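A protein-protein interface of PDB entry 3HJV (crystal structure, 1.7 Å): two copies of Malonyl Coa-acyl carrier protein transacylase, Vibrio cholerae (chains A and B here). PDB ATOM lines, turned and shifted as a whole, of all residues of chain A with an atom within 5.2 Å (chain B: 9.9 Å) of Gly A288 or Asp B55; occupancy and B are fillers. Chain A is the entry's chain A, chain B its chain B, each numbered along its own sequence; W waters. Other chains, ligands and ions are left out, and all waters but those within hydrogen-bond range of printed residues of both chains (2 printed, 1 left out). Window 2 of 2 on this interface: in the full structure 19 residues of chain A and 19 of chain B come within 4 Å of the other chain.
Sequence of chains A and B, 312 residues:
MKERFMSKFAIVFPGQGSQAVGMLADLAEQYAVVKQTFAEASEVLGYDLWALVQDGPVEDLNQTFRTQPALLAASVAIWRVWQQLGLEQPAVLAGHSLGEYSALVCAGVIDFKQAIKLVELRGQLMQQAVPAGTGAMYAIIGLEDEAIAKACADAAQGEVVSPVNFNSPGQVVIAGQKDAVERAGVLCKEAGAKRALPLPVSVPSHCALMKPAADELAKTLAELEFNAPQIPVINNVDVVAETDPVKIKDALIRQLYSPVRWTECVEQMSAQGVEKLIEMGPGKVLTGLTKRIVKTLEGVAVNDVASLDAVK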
ATOM      1  N   LYS A 284      28.285 -36.309  -2.294  1.00  0.00           N
ATOM      2  CA  LYS A 284      29.062 -35.368  -3.109  1.00  0.00           C
ATOM      3  C   LYS A 284      29.227 -34.040  -2.403  1.00  0.00           C
ATOM      4  O   LYS A 284      29.402 -33.018  -3.052  1.00  0.00           O
ATOM      5  CB  LYS A 284      28.351 -35.121  -4.454  1.00  0.00           C
ATOM      6  CG  LYS A 284      28.379 -36.265  -5.391  1.00  0.00           C
ATOM      7  CD  LYS A 284      27.884 -35.802  -6.775  1.00  0.00           C
ATOM      8  CE  LYS A 284      28.211 -36.802  -7.860  1.00  0.00           C
ATOM      9  NZ  LYS A 284      27.778 -38.180  -7.503  1.00  0.00           N
ATOM     10  N   VAL A 285      29.184 -34.046  -1.067  1.00  0.00           N
ATOM     11  CA  VAL A 285      29.258 -32.807  -0.299  1.00  0.00           C
ATOM     12  C   VAL A 285      30.548 -31.993  -0.539  1.00  0.00           C
ATOM     13  O   VAL A 285      30.496 -30.803  -0.848  1.00  0.00           O
ATOM     14  CB  VAL A 285      29.094 -33.062   1.212  1.00  0.00           C
ATOM     15  CG1 VAL A 285      29.284 -31.786   1.973  1.00  0.00           C
ATOM     16  CG2 VAL A 285      27.702 -33.665   1.481  1.00  0.00           C
ATOM     17  N   LEU A 286      31.700 -32.632  -0.422  1.00  0.00           N
ATOM     18  CA  LEU A 286      32.962 -31.913  -0.611  1.00  0.00           C
ATOM     19  C   LEU A 286      33.190 -31.481  -2.045  1.00  0.00           C
ATOM     20  O   LEU A 286      33.876 -30.508  -2.278  1.00  0.00           O
ATOM     21  CB  LEU A 286      34.169 -32.719  -0.133  1.00  0.00           C
ATOM     22  CG  LEU A 286      34.199 -33.068   1.336  1.00  0.00           C
ATOM     23  CD1 LEU A 286      35.461 -33.859   1.668  1.00  0.00           C
ATOM     24  CD2 LEU A 286      34.096 -31.819   2.251  1.00  0.00           C
ATOM     25  N   THR A 287      32.602 -32.206  -2.991  1.00  0.00           N
ATOM     26  CA  THR A 287      32.731 -31.879  -4.405  1.00  0.00           C
ATOM     27  C   THR A 287      32.139 -30.471  -4.639  1.00  0.00           C
ATOM     28  O   THR A 287      32.724 -29.626  -5.335  1.00  0.00           O
ATOM     29  CB  THR A 287      32.109 -32.993  -5.282  1.00  0.00           C
ATOM     30  OG1 THR A 287      32.751 -34.243  -4.985  1.00  0.00           O
ATOM     31  CG2 THR A 287      32.257 -32.680  -6.771  1.00  0.00           C
ATOM     32  N   GLY A 288      30.995 -30.197  -4.003  1.00  0.00           N
ATOM     33  CA  GLY A 288      30.359 -28.885  -4.077  1.00  0.00           C
ATOM     34  C   GLY A 288      31.124 -27.748  -3.417  1.00  0.00           C
ATOM     35  O   GLY A 288      31.066 -26.607  -3.885  1.00  0.00           O
ATOM     36  N   LEU A 289      31.828 -28.026  -2.327  1.00  0.00           N
ATOM     37  CA  LEU A 289      32.649 -27.018  -1.687  1.00  0.00           C
ATOM     38  C   LEU A 289      33.845 -26.659  -2.577  1.00  0.00           C
ATOM     39  O   LEU A 289      34.189 -25.498  -2.677  1.00  0.00           O
ATOM     40  CB  LEU A 289      33.181 -27.458  -0.316  1.00  0.00           C
ATOM     41  CG  LEU A 289      32.244 -27.679   0.869  1.00  0.00           C
ATOM     42  CD1 LEU A 289      33.038 -28.078   2.104  1.00  0.00           C
ATOM     43  CD2 LEU A 289      31.434 -26.414   1.110  1.00  0.00           C
ATOM     44  N   THR A 290      34.482 -27.652  -3.213  1.00  0.00           N
ATOM     45  CA  THR A 290      35.653 -27.384  -4.067  1.00  0.00           C
ATOM     46  C   THR A 290      35.320 -26.321  -5.122  1.00  0.00           C
ATOM     47  O   THR A 290      36.066 -25.354  -5.308  1.00  0.00           O
ATOM     48  CB  THR A 290      36.144 -28.642  -4.785  1.00  0.00           C
ATOM     49  OG1 THR A 290      36.389 -29.668  -3.817  1.00  0.00           O
ATOM     50  CG2 THR A 290      37.427 -28.342  -5.580  1.00  0.00           C
ATOM     51  N   LYS A 291      34.163 -26.502  -5.761  1.00  0.00           N
ATOM     52  CA  LYS A 291      33.628 -25.586  -6.758  1.00  0.00           C
ATOM     53  C   LYS A 291      33.617 -24.142  -6.260  1.00  0.00           C
ATOM     54  O   LYS A 291      33.906 -23.203  -7.005  1.00  0.00           O
ATOM     55  CB  LYS A 291      32.192 -26.059  -7.091  1.00  0.00           C
ATOM     56  CG  LYS A 291      31.413 -25.247  -8.087  1.00  0.00           C
ATOM     57  CD  LYS A 291      30.116 -25.969  -8.468  1.00  0.00           C
ATOM     58  CE  LYS A 291      29.245 -25.091  -9.358  1.00  0.00           C
ATOM     59  NZ  LYS A 291      27.993 -25.783  -9.773  1.00  0.00           N
ATOM     60  N   ARG A 292      33.291 -23.963  -4.986  1.00  0.00           N
ATOM     61  CA  ARG A 292      33.205 -22.634  -4.386  1.00  0.00           C
ATOM     62  C   ARG A 292      34.507 -22.069  -3.815  1.00  0.00           C
ATOM     63  O   ARG A 292      34.539 -20.912  -3.364  1.00  0.00           O
ATOM     64  CB  ARG A 292      32.105 -22.646  -3.317  1.00  0.00           C
ATOM     65  CG  ARG A 292      30.745 -22.994  -3.903  1.00  0.00           C
ATOM     66  CD  ARG A 292      29.555 -22.741  -2.952  1.00  0.00           C
ATOM     67  NE  ARG A 292      29.354 -23.743  -1.903  1.00  0.00           N
ATOM     68  CZ  ARG A 292      28.627 -24.873  -2.014  1.00  0.00           C
ATOM     69  NH1 ARG A 292      28.014 -25.206  -3.159  1.00  0.00           N
ATOM     70  NH2 ARG A 292      28.511 -25.694  -0.968  1.00  0.00           N
ATOM     71  N   ALA B  20      20.136 -36.218  -0.167  1.00  0.00           N
ATOM     72  CA  ALA B  20      21.577 -36.275  -0.202  1.00  0.00           C
ATOM     73  C   ALA B  20      22.067 -35.410  -1.337  1.00  0.00           C
ATOM     74  O   ALA B  20      21.506 -35.427  -2.422  1.00  0.00           O
ATOM     75  CB  ALA B  20      22.064 -37.706  -0.417  1.00  0.00           C
ATOM     76  N   VAL B  21      23.151 -34.682  -1.102  1.00  0.00           N
ATOM     77  CA  VAL B  21      23.772 -33.905  -2.180  1.00  0.00           C
ATOM     78  C   VAL B  21      24.264 -34.887  -3.239  1.00  0.00           C
ATOM     79  O   VAL B  21      24.963 -35.874  -2.934  1.00  0.00           O
ATOM     80  CB  VAL B  21      24.935 -33.009  -1.662  1.00  0.00           C
ATOM     81  CG1 VAL B  21      25.682 -32.338  -2.832  1.00  0.00           C
ATOM     82  CG2 VAL B  21      24.377 -31.933  -0.726  1.00  0.00           C
ATOM     83  N   GLY B  22      23.886 -34.635  -4.490  1.00  0.00           N
ATOM     84  CA  GLY B  22      24.270 -35.486  -5.590  1.00  0.00           C
ATOM     85  C   GLY B  22      23.226 -36.509  -5.989  1.00  0.00           C
ATOM     86  O   GLY B  22      23.420 -37.229  -6.966  1.00  0.00           O
ATOM     87  N   MET B  23      22.126 -36.591  -5.244  1.00  0.00           N
ATOM     88  CA  MET B  23      21.084 -37.554  -5.552  1.00  0.00           C
ATOM     89  C   MET B  23      20.558 -37.398  -6.976  1.00  0.00           C
ATOM     90  O   MET B  23      20.457 -36.277  -7.488  1.00  0.00           O
ATOM     91  CB  MET B  23      19.919 -37.440  -4.561  1.00  0.00           C
ATOM     92  CG  MET B  23      19.205 -36.172  -4.581  1.00  0.00           C
ATOM     93  SD  MET B  23      17.774 -36.218  -3.232  1.00  0.00           S
ATOM     94  CE  MET B  23      17.064 -34.450  -3.440  1.00  0.00           C
ATOM     95  N   ALA B  25      21.841 -37.995  -9.807  1.00  0.00           N
ATOM     96  CA  ALA B  25      22.786 -37.643 -10.877  1.00  0.00           C
ATOM     97  C   ALA B  25      22.824 -38.690 -12.015  1.00  0.00           C
ATOM     98  O   ALA B  25      22.672 -38.355 -13.186  1.00  0.00           O
ATOM     99  CB  ALA B  25      24.199 -37.433 -10.307  1.00  0.00           C
ATOM    100  N   ASP B  48      17.120 -22.390  -8.454  1.00  0.00           N
ATOM    101  CA  ASP B  48      17.482 -23.610  -9.166  1.00  0.00           C
ATOM    102  C   ASP B  48      17.589 -24.766  -8.201  1.00  0.00           C
ATOM    103  O   ASP B  48      18.637 -24.960  -7.575  1.00  0.00           O
ATOM    104  CB  ASP B  48      18.817 -23.411  -9.864  1.00  0.00           C
ATOM    105  CG  ASP B  48      19.161 -24.521 -10.838  1.00  0.00           C
ATOM    106  OD1 ASP B  48      18.596 -25.627 -10.781  1.00  0.00           O
ATOM    107  OD2 ASP B  48      20.042 -24.271 -11.688  1.00  0.00           O
ATOM    108  N   LEU B  49      16.515 -25.547  -8.134  1.00  0.00           N
ATOM    109  CA  LEU B  49      16.442 -26.667  -7.221  1.00  0.00           C
ATOM    110  C   LEU B  49      17.424 -27.789  -7.567  1.00  0.00           C
ATOM    111  O   LEU B  49      17.976 -28.423  -6.652  1.00  0.00           O
ATOM    112  CB  LEU B  49      15.021 -27.206  -7.196  1.00  0.00           C
ATOM    113  CG  LEU B  49      14.702 -28.277  -6.161  1.00  0.00           C
ATOM    114  CD1 LEU B  49      14.923 -27.775  -4.707  1.00  0.00           C
ATOM    115  CD2 LEU B  49      13.279 -28.771  -6.380  1.00  0.00           C
ATOM    116  N   TRP B  50      17.633 -28.035  -8.865  1.00  0.00           N
ATOM    117  CA  TRP B  50      18.581 -29.068  -9.326  1.00  0.00           C
ATOM    118  C   TRP B  50      19.988 -28.729  -8.883  1.00  0.00           C
ATOM    119  O   TRP B  50      20.704 -29.596  -8.356  1.00  0.00           O
ATOM    120  CB  TRP B  50      18.504 -29.266 -10.837  1.00  0.00           C
ATOM    121  CG  TRP B  50      19.358 -30.395 -11.363  1.00  0.00           C
ATOM    122  CD1 TRP B  50      20.372 -30.284 -12.240  1.00  0.00           C
ATOM    123  CD2 TRP B  50      19.260 -31.787 -11.038  1.00  0.00           C
ATOM    124  NE1 TRP B  50      20.944 -31.506 -12.471  1.00  0.00           N
ATOM    125  CE2 TRP B  50      20.272 -32.452 -11.759  1.00  0.00           C
ATOM    126  CE3 TRP B  50      18.439 -32.536 -10.196  1.00  0.00           C
ATOM    127  CZ2 TRP B  50      20.456 -33.825 -11.694  1.00  0.00           C
ATOM    128  CZ3 TRP B  50      18.619 -33.929 -10.120  1.00  0.00           C
ATOM    129  CH2 TRP B  50      19.627 -34.549 -10.866  1.00  0.00           C
ATOM    130  N   ALA B  51      20.368 -27.465  -9.051  1.00  0.00           N
ATOM    131  CA  ALA B  51      21.692 -27.002  -8.633  1.00  0.00           C
ATOM    132  C   ALA B  51      21.873 -27.162  -7.124  1.00  0.00           C
ATOM    133  O   ALA B  51      22.928 -27.622  -6.677  1.00  0.00           O
ATOM    134  CB  ALA B  51      21.926 -25.559  -9.060  1.00  0.00           C
ATOM    135  N   LEU B  52      20.845 -26.844  -6.338  1.00  0.00           N
ATOM    136  CA  LEU B  52      20.924 -27.030  -4.873  1.00  0.00           C
ATOM    137  C   LEU B  52      21.147 -28.496  -4.498  1.00  0.00           C
ATOM    138  O   LEU B  52      21.981 -28.829  -3.636  1.00  0.00           O
ATOM    139  CB  LEU B  52      19.662 -26.482  -4.174  1.00  0.00           C
ATOM    140  CG  LEU B  52      19.519 -26.735  -2.659  1.00  0.00           C
ATOM    141  CD1 LEU B  52      20.686 -26.146  -1.866  1.00  0.00           C
ATOM    142  CD2 LEU B  52      18.149 -26.231  -2.129  1.00  0.00           C
ATOM    143  N   VAL B  53      20.402 -29.378  -5.153  1.00  0.00           N
ATOM    144  CA  VAL B  53      20.493 -30.802  -4.890  1.00  0.00           C
ATOM    145  C   VAL B  53      21.848 -31.388  -5.300  1.00  0.00           C
ATOM    146  O   VAL B  53      22.374 -32.249  -4.600  1.00  0.00           O
ATOM    147  CB  VAL B  53      19.322 -31.539  -5.569  1.00  0.00           C
ATOM    148  CG1 VAL B  53      19.544 -33.022  -5.622  1.00  0.00           C
ATOM    149  CG2 VAL B  53      17.976 -31.192  -4.872  1.00  0.00           C
ATOM    150  N   GLN B  54      22.402 -30.933  -6.418  1.00  0.00           N
ATOM    151  CA  GLN B  54      23.681 -31.445  -6.899  1.00  0.00           C
ATOM    152  C   GLN B  54      24.898 -30.839  -6.227  1.00  0.00           C
ATOM    153  O   GLN B  54      25.912 -31.505  -6.100  1.00  0.00           O
ATOM    154  CB  GLN B  54      23.806 -31.239  -8.406  1.00  0.00           C
ATOM    155  CG  GLN B  54      22.756 -32.015  -9.200  1.00  0.00           C
ATOM    156  CD  GLN B  54      22.743 -33.488  -8.830  1.00  0.00           C
ATOM    157  OE1 GLN B  54      23.781 -34.147  -8.832  1.00  0.00           O
ATOM    158  NE2 GLN B  54      21.573 -34.006  -8.520  1.00  0.00           N
ATOM    159  N   ASP B  55      24.812 -29.573  -5.843  1.00  0.00           N
ATOM    160  CA  ASP B  55      25.967 -28.850  -5.311  1.00  0.00           C
ATOM    161  C   ASP B  55      25.933 -28.485  -3.838  1.00  0.00           C
ATOM    162  O   ASP B  55      26.989 -28.289  -3.235  1.00  0.00           O
ATOM    163  CB  ASP B  55      26.131 -27.525  -6.066  1.00  0.00           C
ATOM    164  CG  ASP B  55      26.351 -27.706  -7.558  1.00  0.00           C
ATOM    165  OD1 ASP B  55      26.838 -28.777  -7.985  1.00  0.00           O
ATOM    166  OD2 ASP B  55      26.051 -26.753  -8.294  1.00  0.00           O
ATOM    167  N   GLY B  56      24.737 -28.363  -3.278  1.00  0.00           N
ATOM    168  CA  GLY B  56      24.564 -27.833  -1.931  1.00  0.00           C
ATOM    169  C   GLY B  56      24.354 -26.332  -2.070  1.00  0.00           C
ATOM    170  O   GLY B  56      24.110 -25.840  -3.182  1.00  0.00           O
ATOM    171  N   PRO B  57      24.566 -25.565  -0.988  1.00  0.00           N
ATOM    172  CA  PRO B  57      25.073 -25.996   0.300  1.00  0.00           C
ATOM    173  C   PRO B  57      24.151 -26.970   0.993  1.00  0.00           C
ATOM    174  O   PRO B  57      22.917 -26.833   0.927  1.00  0.00           O
ATOM    175  CB  PRO B  57      25.180 -24.691   1.108  1.00  0.00           C
ATOM    176  CG  PRO B  57      25.030 -23.621   0.157  1.00  0.00           C
ATOM    177  CD  PRO B  57      24.233 -24.131  -0.980  1.00  0.00           C
ATOM    178  N   VAL B  58      24.717 -27.959   1.671  1.00  0.00           N
ATOM    179  CA  VAL B  58      23.884 -28.977   2.285  1.00  0.00           C
ATOM    180  C   VAL B  58      23.044 -28.419   3.439  1.00  0.00           C
ATOM    181  O   VAL B  58      21.925 -28.892   3.672  1.00  0.00           O
ATOM    182  CB  VAL B  58      24.700 -30.189   2.739  1.00  0.00           C
ATOM    183  CG1 VAL B  58      25.663 -29.784   3.859  1.00  0.00           C
ATOM    184  CG2 VAL B  58      23.768 -31.316   3.184  1.00  0.00           C
ATOM    185  N   GLU B  59      23.549 -27.393   4.132  1.00  0.00           N
ATOM    186  CA  GLU B  59      22.788 -26.811   5.229  1.00  0.00           C
ATOM    187  C   GLU B  59      21.487 -26.212   4.718  1.00  0.00           C
ATOM    188  O   GLU B  59      20.475 -26.299   5.394  1.00  0.00           O
ATOM    189  CB  GLU B  59      23.605 -25.807   6.055  1.00  0.00           C
ATOM    190  CG  GLU B  59      24.873 -26.381   6.690  1.00  0.00           C
ATOM    191  CD  GLU B  59      26.126 -26.267   5.810  1.00  0.00           C
ATOM    192  OE1 GLU B  59      26.011 -26.014   4.570  1.00  0.00           O
ATOM    193  OE2 GLU B  59      27.243 -26.363   6.386  1.00  0.00           O
ATOM    194  N   ASP B  60      21.512 -25.653   3.517  1.00  0.00           N
ATOM    195  CA  ASP B  60      20.302 -25.137   2.881  1.00  0.00           C
ATOM    196  C   ASP B  60      19.393 -26.269   2.403  1.00  0.00           C
ATOM    197  O   ASP B  60      18.165 -26.213   2.593  1.00  0.00           O
ATOM    198  CB  ASP B  60      20.670 -24.266   1.694  1.00  0.00           C
ATOM    199  CG  ASP B  60      21.323 -22.948   2.108  1.00  0.00           C
ATOM    200  OD1 ASP B  60      20.593 -22.061   2.611  1.00  0.00           O
ATOM    201  OD2 ASP B  60      22.545 -22.775   1.888  1.00  0.00           O
ATOM    202  N   LEU B  61      19.974 -27.322   1.821  1.00  0.00           N
ATOM    203  CA  LEU B  61      19.167 -28.458   1.374  1.00  0.00           C
ATOM    204  C   LEU B  61      18.437 -29.110   2.539  1.00  0.00           C
ATOM    205  O   LEU B  61      17.345 -29.632   2.357  1.00  0.00           O
ATOM    206  CB  LEU B  61      20.031 -29.523   0.677  1.00  0.00           C
ATOM    207  CG  LEU B  61      19.340 -30.783   0.147  1.00  0.00           C
ATOM    208  CD1 LEU B  61      18.319 -30.466  -0.950  1.00  0.00           C
ATOM    209  CD2 LEU B  61      20.415 -31.723  -0.370  1.00  0.00           C
HETATM  210  O   HOH W   1      28.356 -31.737  -5.342  1.00  0.00           O
HETATM  211  O   HOH W   2      28.401 -29.065  -0.966  1.00  0.00           O
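No position is printed for both chains. Of the 7 pairs that touch across the chains among the printed residues, none has its exchanged pair printed and touching as well.
Printed residues of chain B within 4 Å of Lys A284: Val B21 (3.4 Å) and Gly B22 (3.8 Å). Of chain B, only Asp B55 comes within 4 Å of Gly A288. Lys A291 touches just one residue of chain B: Asp B55. Of the printed residues of chain A, Gly B22 touches Lys A284. Leu B49 touches none of the printed residues of chain A. Asp B55 touches three residues of chain A. Printed residues of chain A within 4 Å of Gly B56: Arg A292. Leu B61 touches none of the printed residues of chain A.
Water W1 lies within hydrogen-bond range of O of Gln B54 (2.6 Å), O of Lys A284 (2.8 Å) and N of Gly A288 (3.3 Å). Water W2 lies within hydrogen-bond range of the backbone carbonyl oxygen of Val A285 (2.7 Å), the backbone carbonyl oxygen of Asp B55 (2.8 Å) and the guanidinium group of Arg A292 (3.4 Å).
Among the printed residues, merely in contact across the chains: Gly A288 with Asp B55 (3.5 Å), Arg A292 with Pro B57 (3.7 Å), Lys A284 with Gly B22 (3.8 Å) and Arg A292 with Gly B56 (3.96 Å).
O of Val B53 lies within hydrogen-bond range of N of Gly B22. O of Gly A288 is in hydrogen-bond range of NH1 of Arg A292, 3.4 Å away.
The backbone NH (N) of Lys A284 sits at hydrogen-bond distance from the backbone carbonyl oxygen (O) of Val B21, at 3.4 Å. NZ of Lys A291 is in salt-bridge range of OD2 of Asp B55. The guanidinium group (NH1) of Arg A292 sits at hydrogen-bond distance from the backbone carbonyl oxygen (O) of Asp B55 (3.2 Å).
Of the 19 printed residues of chain B, 5 touch a printed residue of chain A. Printed residues of chain B that touch a printed residue of chain A: Val B21, Gly B22, Asp B55, Gly B56 and Pro B57. Among the printed residues, Asp or Glu carboxylates within 4 Å of a Lys or Arg side-chain nitrogen of the other chain: Lys A291 with Asp B55 (2.6 Å).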
